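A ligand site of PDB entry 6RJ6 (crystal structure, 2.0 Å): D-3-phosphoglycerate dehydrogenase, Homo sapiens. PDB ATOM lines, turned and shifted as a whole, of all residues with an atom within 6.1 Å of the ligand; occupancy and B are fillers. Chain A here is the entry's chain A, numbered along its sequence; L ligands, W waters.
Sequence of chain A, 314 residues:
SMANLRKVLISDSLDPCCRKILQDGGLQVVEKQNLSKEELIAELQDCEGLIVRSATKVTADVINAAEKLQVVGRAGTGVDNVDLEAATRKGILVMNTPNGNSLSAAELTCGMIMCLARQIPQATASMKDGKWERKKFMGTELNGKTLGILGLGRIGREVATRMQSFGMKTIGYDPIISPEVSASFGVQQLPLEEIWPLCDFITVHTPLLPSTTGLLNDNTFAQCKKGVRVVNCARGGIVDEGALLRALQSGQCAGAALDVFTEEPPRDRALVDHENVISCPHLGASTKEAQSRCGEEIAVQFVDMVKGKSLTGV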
ATOM      1  N   ASN A  99     -39.574 -10.357  -6.420  1.00  0.00           N
ATOM      2  CA  ASN A  99     -40.022  -9.313  -7.339  1.00  0.00           C
ATOM      3  C   ASN A  99     -41.056  -8.360  -6.717  1.00  0.00           C
ATOM      4  O   ASN A  99     -40.963  -7.154  -6.923  1.00  0.00           O
ATOM      5  CB  ASN A  99     -40.553  -9.916  -8.644  1.00  0.00           C
ATOM      6  CG  ASN A  99     -39.474 -10.261  -9.646  1.00  0.00           C
ATOM      7  OD1 ASN A  99     -38.640 -11.143  -9.428  1.00  0.00           O
ATOM      8  ND2 ASN A  99     -39.492  -9.586 -10.785  1.00  0.00           N
ATOM      9  N   SER A 102     -39.232  -6.733  -2.859  1.00  0.00           N
ATOM     10  CA  SER A 102     -37.797  -6.756  -3.143  1.00  0.00           C
ATOM     11  C   SER A 102     -37.104  -5.425  -2.805  1.00  0.00           C
ATOM     12  O   SER A 102     -36.118  -5.412  -2.066  1.00  0.00           O
ATOM     13  CB  SER A 102     -37.527  -7.145  -4.585  1.00  0.00           C
ATOM     14  OG  SER A 102     -37.875  -8.498  -4.823  1.00  0.00           O
ATOM     15  N   ILE A 149     -21.394  -8.798  -1.216  1.00  0.00           N
ATOM     16  CA  ILE A 149     -22.794  -9.204  -1.404  1.00  0.00           C
ATOM     17  C   ILE A 149     -22.886 -10.683  -1.802  1.00  0.00           C
ATOM     18  O   ILE A 149     -22.693 -11.017  -2.975  1.00  0.00           O
ATOM     19  CB  ILE A 149     -23.594  -8.258  -2.352  1.00  0.00           C
ATOM     20  CG1 ILE A 149     -23.311  -6.765  -2.065  1.00  0.00           C
ATOM     21  CG2 ILE A 149     -25.099  -8.562  -2.292  1.00  0.00           C
ATOM     22  CD1 ILE A 149     -23.346  -5.836  -3.268  1.00  0.00           C
ATOM     23  N   LEU A 150     -23.183 -11.546  -0.830  1.00  0.00           N
ATOM     24  CA  LEU A 150     -23.350 -12.991  -1.014  1.00  0.00           C
ATOM     25  C   LEU A 150     -24.815 -13.260  -1.308  1.00  0.00           C
ATOM     26  O   LEU A 150     -25.668 -13.144  -0.418  1.00  0.00           O
ATOM     27  CB  LEU A 150     -22.866 -13.766   0.223  1.00  0.00           C
ATOM     28  CG  LEU A 150     -21.491 -13.386   0.814  1.00  0.00           C
ATOM     29  CD1 LEU A 150     -21.274 -14.059   2.138  1.00  0.00           C
ATOM     30  CD2 LEU A 150     -20.347 -13.694  -0.156  1.00  0.00           C
ATOM     31  N   GLY A 151     -25.099 -13.559  -2.572  1.00  0.00           N
ATOM     32  CA  GLY A 151     -26.438 -13.751  -3.111  1.00  0.00           C
ATOM     33  C   GLY A 151     -26.741 -12.562  -4.005  1.00  0.00           C
ATOM     34  O   GLY A 151     -26.902 -11.442  -3.508  1.00  0.00           O
ATOM     35  N   LEU A 152     -26.739 -12.791  -5.322  1.00  0.00           N
ATOM     36  CA  LEU A 152     -26.915 -11.688  -6.272  1.00  0.00           C
ATOM     37  C   LEU A 152     -28.214 -11.796  -7.068  1.00  0.00           C
ATOM     38  O   LEU A 152     -28.225 -11.598  -8.288  1.00  0.00           O
ATOM     39  CB  LEU A 152     -25.676 -11.545  -7.176  1.00  0.00           C
ATOM     40  CG  LEU A 152     -24.310 -11.359  -6.489  1.00  0.00           C
ATOM     41  CD1 LEU A 152     -23.183 -11.632  -7.453  1.00  0.00           C
ATOM     42  CD2 LEU A 152     -24.165  -9.964  -5.886  1.00  0.00           C
ATOM     43  N   GLY A 153     -29.305 -12.042  -6.360  1.00  0.00           N
ATOM     44  CA  GLY A 153     -30.632 -12.117  -6.940  1.00  0.00           C
ATOM     45  C   GLY A 153     -31.214 -10.723  -7.128  1.00  0.00           C
ATOM     46  O   GLY A 153     -30.472  -9.757  -7.320  1.00  0.00           O
ATOM     47  N   ARG A 154     -32.552 -10.621  -7.052  1.00  0.00           N
ATOM     48  CA  ARG A 154     -33.301  -9.374  -7.189  1.00  0.00           C
ATOM     49  C   ARG A 154     -32.943  -8.364  -6.074  1.00  0.00           C
ATOM     50  O   ARG A 154     -32.721  -7.198  -6.382  1.00  0.00           O
ATOM     51  CB  ARG A 154     -34.817  -9.663  -7.228  1.00  0.00           C
ATOM     52  CG  ARG A 154     -35.718  -8.453  -7.439  1.00  0.00           C
ATOM     53  CD  ARG A 154     -35.936  -8.081  -8.896  1.00  0.00           C
ATOM     54  NE  ARG A 154     -37.007  -7.092  -9.043  1.00  0.00           N
ATOM     55  CZ  ARG A 154     -36.843  -5.777  -8.944  1.00  0.00           C
ATOM     56  NH1 ARG A 154     -37.873  -4.958  -9.096  1.00  0.00           N
ATOM     57  NH2 ARG A 154     -35.637  -5.270  -8.715  1.00  0.00           N
ATOM     58  N   ILE A 155     -32.883  -8.819  -4.808  1.00  0.00           N
ATOM     59  CA  ILE A 155     -32.545  -7.976  -3.643  1.00  0.00           C
ATOM     60  C   ILE A 155     -31.074  -7.510  -3.751  1.00  0.00           C
ATOM     61  O   ILE A 155     -30.822  -6.313  -3.693  1.00  0.00           O
ATOM     62  CB  ILE A 155     -32.794  -8.703  -2.278  1.00  0.00           C
ATOM     63  CG1 ILE A 155     -34.130  -9.502  -2.273  1.00  0.00           C
ATOM     64  CG2 ILE A 155     -32.669  -7.723  -1.075  1.00  0.00           C
ATOM     65  CD1 ILE A 155     -35.350  -8.919  -1.669  1.00  0.00           C
ATOM     66  N   GLY A 156     -30.154  -8.461  -3.929  1.00  0.00           N
ATOM     67  CA  GLY A 156     -28.714  -8.217  -4.022  1.00  0.00           C
ATOM     68  C   GLY A 156     -28.257  -7.189  -5.031  1.00  0.00           C
ATOM     69  O   GLY A 156     -27.300  -6.451  -4.757  1.00  0.00           O
ATOM     70  N   ARG A 157     -28.896  -7.133  -6.225  1.00  0.00           N
ATOM     71  CA  ARG A 157     -28.518  -6.182  -7.266  1.00  0.00           C
ATOM     72  C   ARG A 157     -29.002  -4.762  -6.959  1.00  0.00           C
ATOM     73  O   ARG A 157     -28.284  -3.806  -7.270  1.00  0.00           O
ATOM     74  CB  ARG A 157     -28.933  -6.649  -8.685  1.00  0.00           C
ATOM     75  CG  ARG A 157     -30.420  -6.860  -8.927  1.00  0.00           C
ATOM     76  CD  ARG A 157     -30.694  -7.276 -10.370  1.00  0.00           C
ATOM     77  NE  ARG A 157     -30.095  -8.570 -10.689  1.00  0.00           N
ATOM     78  CZ  ARG A 157     -30.758  -9.720 -10.738  1.00  0.00           C
ATOM     79  NH1 ARG A 157     -30.129 -10.846 -11.035  1.00  0.00           N
ATOM     80  NH2 ARG A 157     -32.070  -9.750 -10.505  1.00  0.00           N
ATOM     81  N   TYR A 173     -20.552 -12.845  -4.648  1.00  0.00           N
ATOM     82  CA  TYR A 173     -20.609 -14.205  -5.154  1.00  0.00           C
ATOM     83  C   TYR A 173     -22.045 -14.667  -5.320  1.00  0.00           C
ATOM     84  O   TYR A 173     -22.939 -14.265  -4.546  1.00  0.00           O
ATOM     85  CB  TYR A 173     -19.848 -15.161  -4.199  1.00  0.00           C
ATOM     86  CG  TYR A 173     -19.928 -16.630  -4.557  1.00  0.00           C
ATOM     87  CD1 TYR A 173     -19.050 -17.201  -5.488  1.00  0.00           C
ATOM     88  CD2 TYR A 173     -20.885 -17.461  -3.988  1.00  0.00           C
ATOM     89  CE1 TYR A 173     -19.148 -18.545  -5.840  1.00  0.00           C
ATOM     90  CE2 TYR A 173     -20.996 -18.801  -4.337  1.00  0.00           C
ATOM     91  CZ  TYR A 173     -20.121 -19.341  -5.254  1.00  0.00           C
ATOM     92  OH  TYR A 173     -20.212 -20.673  -5.595  1.00  0.00           O
ATOM     93  N   ASP A 174     -22.250 -15.538  -6.309  1.00  0.00           N
ATOM     94  CA  ASP A 174     -23.488 -16.233  -6.633  1.00  0.00           C
ATOM     95  C   ASP A 174     -23.136 -17.411  -7.555  1.00  0.00           C
ATOM     96  O   ASP A 174     -22.448 -17.177  -8.560  1.00  0.00           O
ATOM     97  CB  ASP A 174     -24.514 -15.309  -7.289  1.00  0.00           C
ATOM     98  CG  ASP A 174     -25.910 -15.866  -7.226  1.00  0.00           C
ATOM     99  OD1 ASP A 174     -26.222 -16.759  -8.031  1.00  0.00           O
ATOM    100  OD2 ASP A 174     -26.696 -15.406  -6.367  1.00  0.00           O
ATOM    101  N   PRO A 175     -23.529 -18.662  -7.240  1.00  0.00           N
ATOM    102  CA  PRO A 175     -23.190 -19.784  -8.134  1.00  0.00           C
ATOM    103  C   PRO A 175     -23.981 -19.778  -9.445  1.00  0.00           C
ATOM    104  O   PRO A 175     -23.477 -20.265 -10.453  1.00  0.00           O
ATOM    105  CB  PRO A 175     -23.483 -21.025  -7.294  1.00  0.00           C
ATOM    106  CG  PRO A 175     -24.508 -20.593  -6.316  1.00  0.00           C
ATOM    107  CD  PRO A 175     -24.323 -19.126  -6.083  1.00  0.00           C
ATOM    108  N   ILE A 176     -25.204 -19.197  -9.447  1.00  0.00           N
ATOM    109  CA  ILE A 176     -26.085 -19.104 -10.618  1.00  0.00           C
ATOM    110  C   ILE A 176     -25.674 -17.931 -11.510  1.00  0.00           C
ATOM    111  O   ILE A 176     -25.360 -18.149 -12.687  1.00  0.00           O
ATOM    112  CB  ILE A 176     -27.587 -19.047 -10.214  1.00  0.00           C
ATOM    113  CG1 ILE A 176     -28.007 -20.276  -9.347  1.00  0.00           C
ATOM    114  CG2 ILE A 176     -28.499 -18.868 -11.442  1.00  0.00           C
ATOM    115  CD1 ILE A 176     -29.266 -20.112  -8.500  1.00  0.00           C
ATOM    116  N   ILE A 177     -25.702 -16.700 -10.958  1.00  0.00           N
ATOM    117  CA  ILE A 177     -25.372 -15.447 -11.661  1.00  0.00           C
ATOM    118  C   ILE A 177     -23.977 -15.514 -12.269  1.00  0.00           C
ATOM    119  O   ILE A 177     -22.993 -15.746 -11.555  1.00  0.00           O
ATOM    120  CB  ILE A 177     -25.590 -14.185 -10.768  1.00  0.00           C
ATOM    121  CG1 ILE A 177     -27.024 -14.127 -10.152  1.00  0.00           C
ATOM    122  CG2 ILE A 177     -25.226 -12.868 -11.482  1.00  0.00           C
ATOM    123  CD1 ILE A 177     -28.268 -14.031 -11.154  1.00  0.00           C
ATOM    124  N   LEU A 192     -15.682 -17.182  -2.970  1.00  0.00           N
ATOM    125  CA  LEU A 192     -15.968 -16.899  -1.547  1.00  0.00           C
ATOM    126  C   LEU A 192     -14.741 -16.606  -0.666  1.00  0.00           C
ATOM    127  O   LEU A 192     -14.770 -15.620   0.087  1.00  0.00           O
ATOM    128  CB  LEU A 192     -16.794 -18.030  -0.912  1.00  0.00           C
ATOM    129  CG  LEU A 192     -18.276 -18.097  -1.295  1.00  0.00           C
ATOM    130  CD1 LEU A 192     -18.790 -19.516  -1.218  1.00  0.00           C
ATOM    131  CD2 LEU A 192     -19.115 -17.195  -0.401  1.00  0.00           C
ATOM    132  N   HIS A 205     -27.944 -12.168   0.838  1.00  0.00           N
ATOM    133  CA  HIS A 205     -29.204 -12.140   0.079  1.00  0.00           C
ATOM    134  C   HIS A 205     -29.435 -13.433  -0.733  1.00  0.00           C
ATOM    135  O   HIS A 205     -29.666 -13.378  -1.942  1.00  0.00           O
ATOM    136  CB  HIS A 205     -29.284 -10.878  -0.814  1.00  0.00           C
ATOM    137  CG  HIS A 205     -29.164  -9.599  -0.032  1.00  0.00           C
ATOM    138  ND1 HIS A 205     -30.170  -9.177   0.819  1.00  0.00           N
ATOM    139  CD2 HIS A 205     -28.116  -8.744   0.050  1.00  0.00           C
ATOM    140  CE1 HIS A 205     -29.717  -8.063   1.370  1.00  0.00           C
ATOM    141  NE2 HIS A 205     -28.494  -7.765   0.948  1.00  0.00           N
ATOM    142  N   THR A 206     -29.361 -14.575  -0.053  1.00  0.00           N
ATOM    143  CA  THR A 206     -29.573 -15.903  -0.646  1.00  0.00           C
ATOM    144  C   THR A 206     -30.874 -16.486  -0.062  1.00  0.00           C
ATOM    145  O   THR A 206     -31.263 -16.061   1.029  1.00  0.00           O
ATOM    146  CB  THR A 206     -28.390 -16.861  -0.335  1.00  0.00           C
ATOM    147  OG1 THR A 206     -28.514 -17.404   0.981  1.00  0.00           O
ATOM    148  CG2 THR A 206     -27.031 -16.221  -0.505  1.00  0.00           C
ATOM    149  N   PRO A 207     -31.537 -17.498  -0.672  1.00  0.00           N
ATOM    150  CA  PRO A 207     -32.695 -18.102   0.024  1.00  0.00           C
ATOM    151  C   PRO A 207     -32.198 -18.997   1.164  1.00  0.00           C
ATOM    152  O   PRO A 207     -30.999 -19.325   1.197  1.00  0.00           O
ATOM    153  CB  PRO A 207     -33.376 -18.922  -1.076  1.00  0.00           C
ATOM    154  CG  PRO A 207     -32.291 -19.263  -2.027  1.00  0.00           C
ATOM    155  CD  PRO A 207     -31.241 -18.192  -1.944  1.00  0.00           C
ATOM    156  N   LEU A 208     -33.084 -19.371   2.103  1.00  0.00           N
ATOM    157  CA  LEU A 208     -32.685 -20.276   3.170  1.00  0.00           C
ATOM    158  C   LEU A 208     -32.634 -21.693   2.585  1.00  0.00           C
ATOM    159  O   LEU A 208     -33.627 -22.179   2.046  1.00  0.00           O
ATOM    160  CB  LEU A 208     -33.623 -20.202   4.392  1.00  0.00           C
ATOM    161  CG  LEU A 208     -33.337 -21.191   5.546  1.00  0.00           C
ATOM    162  CD1 LEU A 208     -32.060 -20.836   6.299  1.00  0.00           C
ATOM    163  CD2 LEU A 208     -34.518 -21.280   6.494  1.00  0.00           C
ATOM    164  N   LEU A 209     -31.454 -22.306   2.644  1.00  0.00           N
ATOM    165  CA  LEU A 209     -31.150 -23.653   2.156  1.00  0.00           C
ATOM    166  C   LEU A 209     -30.109 -24.283   3.074  1.00  0.00           C
ATOM    167  O   LEU A 209     -29.330 -23.525   3.655  1.00  0.00           O
ATOM    168  CB  LEU A 209     -30.594 -23.585   0.711  1.00  0.00           C
ATOM    169  CG  LEU A 209     -31.505 -23.141  -0.429  1.00  0.00           C
ATOM    170  CD1 LEU A 209     -30.708 -22.907  -1.671  1.00  0.00           C
ATOM    171  CD2 LEU A 209     -32.633 -24.136  -0.682  1.00  0.00           C
ATOM    172  N   SER A 211     -27.273 -25.547   2.401  1.00  0.00           N
ATOM    173  CA  SER A 211     -25.979 -25.113   1.864  1.00  0.00           C
ATOM    174  C   SER A 211     -25.654 -23.668   2.261  1.00  0.00           C
ATOM    175  O   SER A 211     -24.478 -23.318   2.357  1.00  0.00           O
ATOM    176  CB  SER A 211     -25.978 -25.245   0.351  1.00  0.00           C
ATOM    177  OG  SER A 211     -26.965 -24.427  -0.252  1.00  0.00           O
ATOM    178  N   THR A 212     -26.698 -22.824   2.453  1.00  0.00           N
ATOM    179  CA  THR A 212     -26.589 -21.410   2.820  1.00  0.00           C
ATOM    180  C   THR A 212     -26.685 -21.201   4.340  1.00  0.00           C
ATOM    181  O   THR A 212     -26.441 -20.097   4.832  1.00  0.00           O
ATOM    182  CB  THR A 212     -27.615 -20.573   2.032  1.00  0.00           C
ATOM    183  OG1 THR A 212     -28.921 -21.068   2.287  1.00  0.00           O
ATOM    184  CG2 THR A 212     -27.342 -20.565   0.538  1.00  0.00           C
ATOM    185  N   LEU A 215     -23.405 -19.934   6.510  1.00  0.00           N
ATOM    186  CA  LEU A 215     -22.538 -19.350   5.493  1.00  0.00           C
ATOM    187  C   LEU A 215     -21.462 -18.462   6.147  1.00  0.00           C
ATOM    188  O   LEU A 215     -20.309 -18.507   5.736  1.00  0.00           O
ATOM    189  CB  LEU A 215     -23.375 -18.546   4.487  1.00  0.00           C
ATOM    190  CG  LEU A 215     -22.777 -18.301   3.103  1.00  0.00           C
ATOM    191  CD1 LEU A 215     -22.603 -19.596   2.329  1.00  0.00           C
ATOM    192  CD2 LEU A 215     -23.644 -17.330   2.316  1.00  0.00           C
ATOM    193  N   ALA A 234     -32.190 -11.132   5.092  1.00  0.00           N
ATOM    194  CA  ALA A 234     -32.641 -12.215   4.224  1.00  0.00           C
ATOM    195  C   ALA A 234     -33.422 -13.269   5.032  1.00  0.00           C
ATOM    196  O   ALA A 234     -34.641 -13.142   5.157  1.00  0.00           O
ATOM    197  CB  ALA A 234     -31.450 -12.838   3.520  1.00  0.00           C
HETATM  198  C1  LIG L   1     -24.820 -18.373  -2.585  1.00  0.00           C
HETATM  199  C2  LIG L   1     -26.037 -18.618  -3.237  1.00  0.00           C
HETATM  200  C3  LIG L   1     -26.468 -19.958  -3.241  1.00  0.00           C
HETATM  201  C4  LIG L   1     -27.970 -18.762  -4.426  1.00  0.00           C
HETATM  202  C5  LIG L   1     -29.223 -18.490  -5.203  1.00  0.00           C
HETATM  203  N1  LIG L   1     -29.150 -17.473  -6.080  1.00  0.00           N
HETATM  204  C6  LIG L   1     -28.409 -21.279  -4.168  1.00  0.00           C
HETATM  205  C7  LIG L   1     -29.816 -15.783  -7.699  1.00  0.00           C
HETATM  206  C8  LIG L   1     -31.670 -15.034  -3.649  1.00  0.00           C
HETATM  207  C9  LIG L   1     -33.018 -15.334  -3.735  1.00  0.00           C
HETATM  208  C10 LIG L   1     -33.499 -16.126  -4.771  1.00  0.00           C
HETATM  209  C11 LIG L   1     -24.078 -19.372  -1.959  1.00  0.00           C
HETATM  210  C12 LIG L   1     -23.791 -21.824  -1.282  1.00  0.00           C
HETATM  211  C13 LIG L   1     -30.301 -16.830  -6.717  1.00  0.00           C
HETATM  212  C14 LIG L   1     -31.265 -16.263  -5.697  1.00  0.00           C
HETATM  213  C15 LIG L   1     -30.800 -15.497  -4.629  1.00  0.00           C
HETATM  214  C16 LIG L   1     -24.549 -20.699  -1.953  1.00  0.00           C
HETATM  215  C17 LIG L   1     -32.616 -16.585  -5.733  1.00  0.00           C
HETATM  216  C18 LIG L   1     -34.762 -13.206  -3.029  1.00  0.00           C
HETATM  217  C19 LIG L   1     -33.911 -12.482  -4.049  1.00  0.00           C
HETATM  218  C20 LIG L   1     -25.739 -20.974  -2.614  1.00  0.00           C
HETATM  219  C21 LIG L   1     -27.007 -17.875  -3.984  1.00  0.00           C
HETATM  220  N2  LIG L   1     -27.662 -20.043  -3.953  1.00  0.00           N
HETATM  221  O1  LIG L   1     -30.257 -19.135  -5.009  1.00  0.00           O
HETATM  222  O2  LIG L   1     -29.086 -16.375  -8.765  1.00  0.00           O
HETATM  223  O3  LIG L   1     -33.348 -14.546  -1.285  1.00  0.00           O
HETATM  224  O4  LIG L   1     -35.219 -15.706  -2.395  1.00  0.00           O
HETATM  225  O5  LIG L   1     -32.803 -12.022  -3.660  1.00  0.00           O
HETATM  226  O6  LIG L   1     -34.360 -12.363  -5.205  1.00  0.00           O
HETATM  227  S1  LIG L   1     -34.118 -14.781  -2.472  1.00  0.00           S
HETATM  228 CL1  LIG L   1     -24.229 -16.758  -2.607  1.00  0.00          CL
HETATM  229 CL2  LIG L   1     -22.601 -18.996  -1.164  1.00  0.00          CL
HETATM  230  O   HOH W   1     -36.621 -10.810  -4.192  1.00  0.00           O
HETATM  231  O   HOH W   2     -33.502 -14.719   1.636  1.00  0.00           O
HETATM  232  O   HOH W   3     -35.225 -18.756  -3.812  1.00  0.00           O
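An oxygen (O2) of the ligand lies within hydrogen-bond range of the side-chain carboxylate (OD1) of Asp 174 (3.0 Å).
An oxygen (O6) of the ligand lies within hydrogen-bond range of the backbone NH of Arg 154, at 3.1 Å.
An oxygen (O5) of the ligand sits close to the backbone NH of Ile 155, at 3.4 Å.
The side-chain carboxylate (OD1) of Asp 174 lies within hydrogen-bond range of the backbone NH (N) of Ile 177 (3.0 Å).
The side-chain carboxylate (OD1) of Asp 174 lies within hydrogen-bond range of the backbone NH (N) of Ile 176.
The backbone NH of Leu 152 lies within hydrogen-bond range of the side-chain carboxylate of Asp 174 (2.8 Å).
The backbone NH (N) of His 205 is in hydrogen-bond range of the backbone carbonyl oxygen (O) of Leu 150, 2.8 Å away.
The backbone NH of Gly 151 lies within hydrogen-bond range of the backbone carbonyl oxygen of Tyr 173 (3.0 Å).
O of Pro 207 is in hydrogen-bond range of OG1 of Thr 212, 2.9 Å away.
The backbone carbonyl oxygen (O) of Ile 149 lies within hydrogen-bond range of the backbone NH (N) of Tyr 173 (3.3 Å).
The side-chain hydroxyl of Thr 212 lies within hydrogen-bond range of the backbone carbonyl oxygen of Leu 209, at 2.8 Å.
Water W1 bridges OG of Ser 102 (2.7 Å) and O6 of the ligand (2.9 Å).
Water W2 lies within hydrogen-bond range of the backbone carbonyl oxygen of Thr 206 and an oxygen (O3) of the ligand.
O of Thr 206 lies close to O3 of the ligand (3.5 Å).
C of Leu 150 touches CL1 of the ligand, at 3.8 Å.
Gly 151 touches the ligand (N to CL1, 3.3 Å).
CA of Gly 153 touches C7 of the ligand, at 3.8 Å.
O of Tyr 173 touches CL1 of the ligand, at 3.4 Å.
Pro 175 touches the ligand (CD to C2, 3.4 Å).
Ile 176 touches the ligand (CB to O2, 3.4 Å).
Ile 177 touches the ligand.
Leu 192 touches the ligand.
His 205 touches the ligand (O to C8, 3.1 Å).
CD of Pro 207 touches O1 of the ligand, 3.4 Å away.
CD1 of Leu 209 touches C6 of the ligand, 3.8 Å away.
Ser 211 touches the ligand (O to C12, 3.99 Å).
CG2 of Thr 212 touches C20 of the ligand, 3.6 Å away.
Leu 215 touches the ligand.
Hydrophobic or aromatic side chains that line the ligand: Ile 155, Tyr 173, Pro 175, Ile 176, Ile 177, Leu 192, Pro 207, Leu 209 and Leu 215.
18 residues have an atom within 4 Å of the ligand: Leu 150, Gly 151, Gly 153, Arg 154, Ile 155, Tyr 173, Asp 174, Pro 175, Ile 176, Ile 177, Leu 192, His 205, Thr 206, Pro 207, Leu 209, Ser 211, Thr 212 and Leu 215.
The nearest printed residue that does not touch the ligand is Leu 152 (4.3 Å).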
